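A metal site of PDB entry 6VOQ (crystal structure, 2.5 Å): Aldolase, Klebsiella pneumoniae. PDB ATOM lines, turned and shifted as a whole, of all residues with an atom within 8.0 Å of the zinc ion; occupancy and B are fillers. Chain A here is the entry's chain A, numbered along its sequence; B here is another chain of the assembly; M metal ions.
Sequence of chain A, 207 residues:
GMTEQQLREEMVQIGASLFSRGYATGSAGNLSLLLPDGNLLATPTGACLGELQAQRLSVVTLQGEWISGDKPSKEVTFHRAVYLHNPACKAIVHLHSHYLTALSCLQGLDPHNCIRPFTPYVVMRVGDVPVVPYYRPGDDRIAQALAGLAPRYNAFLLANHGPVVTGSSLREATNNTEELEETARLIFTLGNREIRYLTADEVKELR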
ATOM      1  N   SER A  27     -16.397 -29.051  26.650  1.00  0.00           N
ATOM      2  CA  SER A  27     -15.249 -28.261  27.092  1.00  0.00           C
ATOM      3  C   SER A  27     -14.579 -27.486  25.969  1.00  0.00           C
ATOM      4  O   SER A  27     -13.538 -26.876  26.199  1.00  0.00           O
ATOM      5  CB  SER A  27     -14.229 -29.184  27.769  1.00  0.00           C
ATOM      6  OG  SER A  27     -13.463 -29.890  26.795  1.00  0.00           O
ATOM      7  N   ALA A  28     -15.148 -27.490  24.756  1.00  0.00           N
ATOM      8  CA  ALA A  28     -14.472 -26.948  23.582  1.00  0.00           C
ATOM      9  C   ALA A  28     -14.712 -25.449  23.439  1.00  0.00           C
ATOM     10  O   ALA A  28     -15.804 -24.946  23.680  1.00  0.00           O
ATOM     11  CB  ALA A  28     -14.926 -27.661  22.311  1.00  0.00           C
ATOM     12  N   GLY A  29     -13.662 -24.754  23.019  1.00  0.00           N
ATOM     13  CA  GLY A  29     -13.783 -23.358  22.661  1.00  0.00           C
ATOM     14  C   GLY A  29     -13.171 -22.447  23.702  1.00  0.00           C
ATOM     15  O   GLY A  29     -13.066 -22.784  24.887  1.00  0.00           O
ATOM     16  N   ASN A  30     -12.762 -21.265  23.256  1.00  0.00           N
ATOM     17  CA  ASN A  30     -12.268 -20.251  24.165  1.00  0.00           C
ATOM     18  C   ASN A  30     -12.418 -18.874  23.520  1.00  0.00           C
ATOM     19  O   ASN A  30     -12.491 -18.755  22.295  1.00  0.00           O
ATOM     20  CB  ASN A  30     -10.811 -20.517  24.551  1.00  0.00           C
ATOM     21  CG  ASN A  30      -9.977 -21.009  23.396  1.00  0.00           C
ATOM     22  OD1 ASN A  30      -9.516 -20.217  22.574  1.00  0.00           O
ATOM     23  ND2 ASN A  30      -9.790 -22.319  23.325  1.00  0.00           N
ATOM     24  N   SER A  73      -6.886 -20.778  29.349  1.00  0.00           N
ATOM     25  CA  SER A  73      -6.953 -21.878  28.402  1.00  0.00           C
ATOM     26  C   SER A  73      -5.592 -22.087  27.763  1.00  0.00           C
ATOM     27  O   SER A  73      -4.872 -21.129  27.472  1.00  0.00           O
ATOM     28  CB  SER A  73      -7.989 -21.573  27.334  1.00  0.00           C
ATOM     29  OG  SER A  73      -8.060 -22.632  26.385  1.00  0.00           O
ATOM     30  N   GLU A  75      -5.106 -22.970  24.814  1.00  0.00           N
ATOM     31  CA  GLU A  75      -5.142 -22.477  23.447  1.00  0.00           C
ATOM     32  C   GLU A  75      -4.969 -20.974  23.352  1.00  0.00           C
ATOM     33  O   GLU A  75      -4.833 -20.447  22.232  1.00  0.00           O
ATOM     34  CB  GLU A  75      -6.443 -22.908  22.780  1.00  0.00           C
ATOM     35  CG  GLU A  75      -6.639 -24.404  22.815  1.00  0.00           C
ATOM     36  CD  GLU A  75      -7.813 -24.870  21.990  1.00  0.00           C
ATOM     37  OE1 GLU A  75      -7.578 -25.346  20.853  1.00  0.00           O
ATOM     38  OE2 GLU A  75      -8.960 -24.771  22.482  1.00  0.00           O
ATOM     39  N   PHE A  78      -2.048 -19.607  21.118  1.00  0.00           N
ATOM     40  CA  PHE A  78      -2.113 -19.163  19.736  1.00  0.00           C
ATOM     41  C   PHE A  78      -3.091 -18.011  19.535  1.00  0.00           C
ATOM     42  O   PHE A  78      -3.063 -17.385  18.469  1.00  0.00           O
ATOM     43  CB  PHE A  78      -2.421 -20.336  18.773  1.00  0.00           C
ATOM     44  CG  PHE A  78      -3.782 -21.000  18.951  1.00  0.00           C
ATOM     45  CD1 PHE A  78      -4.961 -20.343  18.640  1.00  0.00           C
ATOM     46  CD2 PHE A  78      -3.853 -22.320  19.339  1.00  0.00           C
ATOM     47  CE1 PHE A  78      -6.175 -20.976  18.794  1.00  0.00           C
ATOM     48  CE2 PHE A  78      -5.073 -22.964  19.486  1.00  0.00           C
ATOM     49  CZ  PHE A  78      -6.233 -22.294  19.209  1.00  0.00           C
ATOM     50  N   HIS A  79      -3.930 -17.702  20.510  1.00  0.00           N
ATOM     51  CA  HIS A  79      -4.597 -16.404  20.531  1.00  0.00           C
ATOM     52  C   HIS A  79      -3.571 -15.283  20.521  1.00  0.00           C
ATOM     53  O   HIS A  79      -3.649 -14.350  19.708  1.00  0.00           O
ATOM     54  CB  HIS A  79      -5.472 -16.273  21.758  1.00  0.00           C
ATOM     55  CG  HIS A  79      -6.768 -17.003  21.669  1.00  0.00           C
ATOM     56  ND1 HIS A  79      -7.988 -16.371  21.856  1.00  0.00           N
ATOM     57  CD2 HIS A  79      -7.056 -18.308  21.455  1.00  0.00           C
ATOM     58  CE1 HIS A  79      -8.962 -17.264  21.731  1.00  0.00           C
ATOM     59  NE2 HIS A  79      -8.425 -18.437  21.489  1.00  0.00           N
ATOM     60  N   HIS A  94     -12.471 -18.652  19.313  1.00  0.00           N
ATOM     61  CA  HIS A  94     -12.071 -19.963  18.848  1.00  0.00           C
ATOM     62  C   HIS A  94     -13.133 -20.969  19.247  1.00  0.00           C
ATOM     63  O   HIS A  94     -13.466 -21.080  20.432  1.00  0.00           O
ATOM     64  CB  HIS A  94     -10.723 -20.382  19.402  1.00  0.00           C
ATOM     65  CG  HIS A  94     -10.396 -21.808  19.118  1.00  0.00           C
ATOM     66  ND1 HIS A  94     -10.356 -22.323  17.838  1.00  0.00           N
ATOM     67  CD2 HIS A  94     -10.139 -22.846  19.950  1.00  0.00           C
ATOM     68  CE1 HIS A  94     -10.052 -23.606  17.893  1.00  0.00           C
ATOM     69  NE2 HIS A  94      -9.923 -23.948  19.160  1.00  0.00           N
ATOM     70  N   LEU A  95     -13.676 -21.682  18.276  1.00  0.00           N
ATOM     71  CA  LEU A  95     -14.697 -22.683  18.516  1.00  0.00           C
ATOM     72  C   LEU A  95     -14.365 -23.928  17.702  1.00  0.00           C
ATOM     73  O   LEU A  95     -13.605 -23.880  16.742  1.00  0.00           O
ATOM     74  CB  LEU A  95     -16.082 -22.186  18.108  1.00  0.00           C
ATOM     75  CG  LEU A  95     -16.657 -20.989  18.831  1.00  0.00           C
ATOM     76  CD1 LEU A  95     -17.858 -20.535  18.058  1.00  0.00           C
ATOM     77  CD2 LEU A  95     -17.023 -21.376  20.256  1.00  0.00           C
ATOM     78  N   HIS A  96     -14.967 -25.044  18.111  1.00  0.00           N
ATOM     79  CA  HIS A  96     -15.032 -26.223  17.248  1.00  0.00           C
ATOM     80  C   HIS A  96     -16.402 -26.311  16.607  1.00  0.00           C
ATOM     81  O   HIS A  96     -17.040 -27.377  16.638  1.00  0.00           O
ATOM     82  CB  HIS A  96     -14.703 -27.485  18.033  1.00  0.00           C
ATOM     83  CG  HIS A  96     -13.384 -27.441  18.722  1.00  0.00           C
ATOM     84  ND1 HIS A  96     -12.926 -28.478  19.518  1.00  0.00           N
ATOM     85  CD2 HIS A  96     -12.415 -26.502  18.744  1.00  0.00           C
ATOM     86  CE1 HIS A  96     -11.738 -28.160  20.003  1.00  0.00           C
ATOM     87  NE2 HIS A  96     -11.407 -26.968  19.552  1.00  0.00           N
ATOM     88  N   THR A 101     -15.474 -26.934  11.573  1.00  0.00           N
ATOM     89  CA  THR A 101     -14.599 -28.052  11.927  1.00  0.00           C
ATOM     90  C   THR A 101     -14.652 -29.138  10.855  1.00  0.00           C
ATOM     91  O   THR A 101     -13.619 -29.713  10.508  1.00  0.00           O
ATOM     92  CB  THR A 101     -15.009 -28.638  13.278  1.00  0.00           C
ATOM     93  OG1 THR A 101     -14.866 -27.657  14.320  1.00  0.00           O
ATOM     94  CG2 THR A 101     -14.158 -29.865  13.630  1.00  0.00           C
ATOM     95  N   PRO A 137      -2.266 -31.006  19.341  1.00  0.00           N
ATOM     96  CA  PRO A 137      -2.644 -29.882  20.214  1.00  0.00           C
ATOM     97  C   PRO A 137      -1.516 -29.510  21.167  1.00  0.00           C
ATOM     98  O   PRO A 137      -0.897 -30.379  21.801  1.00  0.00           O
ATOM     99  CB  PRO A 137      -3.874 -30.418  20.956  1.00  0.00           C
ATOM    100  CG  PRO A 137      -4.481 -31.397  19.992  1.00  0.00           C
ATOM    101  CD  PRO A 137      -3.317 -32.043  19.293  1.00  0.00           C
ATOM    102  N   LEU A 158      -7.867 -23.995  11.381  1.00  0.00           N
ATOM    103  CA  LEU A 158      -6.923 -25.004  11.822  1.00  0.00           C
ATOM    104  C   LEU A 158      -7.403 -26.370  11.346  1.00  0.00           C
ATOM    105  O   LEU A 158      -8.480 -26.823  11.758  1.00  0.00           O
ATOM    106  CB  LEU A 158      -6.782 -24.996  13.340  1.00  0.00           C
ATOM    107  CG  LEU A 158      -6.485 -23.683  14.046  1.00  0.00           C
ATOM    108  CD1 LEU A 158      -6.279 -23.963  15.516  1.00  0.00           C
ATOM    109  CD2 LEU A 158      -5.254 -23.014  13.466  1.00  0.00           C
ATOM    110  N   ASN A 160      -8.295 -30.152  10.818  1.00  0.00           N
ATOM    111  CA  ASN A 160      -8.649 -31.193  11.785  1.00  0.00           C
ATOM    112  C   ASN A 160      -8.866 -30.612  13.178  1.00  0.00           C
ATOM    113  O   ASN A 160      -8.459 -31.194  14.190  1.00  0.00           O
ATOM    114  CB  ASN A 160      -7.600 -32.291  11.841  1.00  0.00           C
ATOM    115  CG  ASN A 160      -7.362 -32.931  10.503  1.00  0.00           C
ATOM    116  OD1 ASN A 160      -6.433 -32.575   9.781  1.00  0.00           O
ATOM    117  ND2 ASN A 160      -8.201 -33.899  10.163  1.00  0.00           N
ATOM    118  N   HIS A 161      -9.510 -29.449  13.250  1.00  0.00           N
ATOM    119  CA  HIS A 161      -9.576 -28.751  14.521  1.00  0.00           C
ATOM    120  C   HIS A 161     -10.769 -27.802  14.559  1.00  0.00           C
ATOM    121  O   HIS A 161     -11.788 -28.131  15.178  1.00  0.00           O
ATOM    122  CB  HIS A 161      -8.285 -27.992  14.758  1.00  0.00           C
ATOM    123  CG  HIS A 161      -8.160 -27.438  16.136  1.00  0.00           C
ATOM    124  ND1 HIS A 161      -6.955 -27.046  16.678  1.00  0.00           N
ATOM    125  CD2 HIS A 161      -9.092 -27.210  17.096  1.00  0.00           C
ATOM    126  CE1 HIS A 161      -7.148 -26.599  17.905  1.00  0.00           C
ATOM    127  NE2 HIS A 161      -8.433 -26.690  18.182  1.00  0.00           N
ATOM    128  N   GLY A 162     -10.643 -26.638  13.932  1.00  0.00           N
ATOM    129  CA  GLY A 162     -11.697 -25.650  13.929  1.00  0.00           C
ATOM    130  C   GLY A 162     -11.238 -24.226  13.641  1.00  0.00           C
ATOM    131  O   GLY A 162     -10.045 -23.969  13.430  1.00  0.00           O
ATOM    132  N   PRO A 163     -12.188 -23.285  13.648  1.00  0.00           N
ATOM    133  CA  PRO A 163     -11.878 -21.903  13.282  1.00  0.00           C
ATOM    134  C   PRO A 163     -11.285 -21.077  14.417  1.00  0.00           C
ATOM    135  O   PRO A 163     -11.538 -21.309  15.602  1.00  0.00           O
ATOM    136  CB  PRO A 163     -13.244 -21.343  12.878  1.00  0.00           C
ATOM    137  CG  PRO A 163     -14.168 -22.083  13.748  1.00  0.00           C
ATOM    138  CD  PRO A 163     -13.640 -23.470  13.800  1.00  0.00           C
ATOM    139  N   VAL A 164     -10.509 -20.075  14.019  1.00  0.00           N
ATOM    140  CA  VAL A 164      -9.993 -19.030  14.892  1.00  0.00           C
ATOM    141  C   VAL A 164     -10.335 -17.714  14.203  1.00  0.00           C
ATOM    142  O   VAL A 164      -9.857 -17.466  13.087  1.00  0.00           O
ATOM    143  CB  VAL A 164      -8.474 -19.158  15.117  1.00  0.00           C
ATOM    144  CG1 VAL A 164      -7.950 -17.957  15.898  1.00  0.00           C
ATOM    145  CG2 VAL A 164      -8.152 -20.458  15.826  1.00  0.00           C
ATOM    146  N   PRO B 120      -8.428 -34.919  17.127  1.00  0.00           N
ATOM    147  CA  PRO B 120      -7.631 -35.515  18.204  1.00  0.00           C
ATOM    148  C   PRO B 120      -8.396 -35.758  19.496  1.00  0.00           C
ATOM    149  O   PRO B 120      -7.921 -36.543  20.326  1.00  0.00           O
ATOM    150  CB  PRO B 120      -6.527 -34.477  18.423  1.00  0.00           C
ATOM    151  CG  PRO B 120      -7.170 -33.201  18.067  1.00  0.00           C
ATOM    152  CD  PRO B 120      -8.104 -33.498  16.922  1.00  0.00           C
ATOM    153  N   TYR B 121      -9.561 -35.153  19.690  1.00  0.00           N
ATOM    154  CA  TYR B 121     -10.098 -35.005  21.032  1.00  0.00           C
ATOM    155  C   TYR B 121     -10.730 -36.292  21.571  1.00  0.00           C
ATOM    156  O   TYR B 121     -10.598 -36.577  22.757  1.00  0.00           O
ATOM    157  CB  TYR B 121     -11.077 -33.837  21.050  1.00  0.00           C
ATOM    158  CG  TYR B 121     -10.394 -32.610  20.502  1.00  0.00           C
ATOM    159  CD1 TYR B 121      -9.394 -31.968  21.243  1.00  0.00           C
ATOM    160  CD2 TYR B 121     -10.689 -32.109  19.234  1.00  0.00           C
ATOM    161  CE1 TYR B 121      -8.728 -30.869  20.754  1.00  0.00           C
ATOM    162  CE2 TYR B 121     -10.023 -30.996  18.725  1.00  0.00           C
ATOM    163  CZ  TYR B 121      -9.046 -30.387  19.503  1.00  0.00           C
ATOM    164  OH  TYR B 121      -8.372 -29.279  19.035  1.00  0.00           O
HETATM  165 ZN    ZN M   1      -9.513 -25.958  19.890  1.00  0.00          ZN
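The zinc ion is bound by NE2 of His 161 (2.1 Å), NE2 of His 96 (2.2 Å), NE2 of His 94 (2.2 Å) and OE1 of Glu 75 (2.2 Å). The zinc ion has four donor atoms within binding distance.
OH of Tyr 121 of chain B touches the zinc ion (3.6 Å). Five residues have an atom within 4 Å of the zinc ion: Glu 75, His 94, His 96, His 161 and Tyr 121 of chain B. The nearest printed residue that does not touch the zinc ion is Phe 78 (5.0 Å).
O of His 94 is in hydrogen-bond range of N of Asn 30, 2.9 Å away. The backbone NH of Glu 75 sits close to the side-chain hydroxyl of Ser 73. A ring nitrogen (NE2) of His 161 sits close to the side-chain hydroxyl (OH) of Tyr 121 of chain B (2.7 Å). O of His 161 sits at hydrogen-bond distance from OG1 of Thr 101. The side-chain carboxylate of Glu 75 lies within hydrogen-bond range of the side-chain amide nitrogen of Asn 30 (2.7 Å). A ring nitrogen (ND1) of His 94 lies within hydrogen-bond range of the backbone carbonyl oxygen of Pro 163 (2.7 Å). OG1 of Thr 101 lies close to O of His 96 (3.2 Å).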
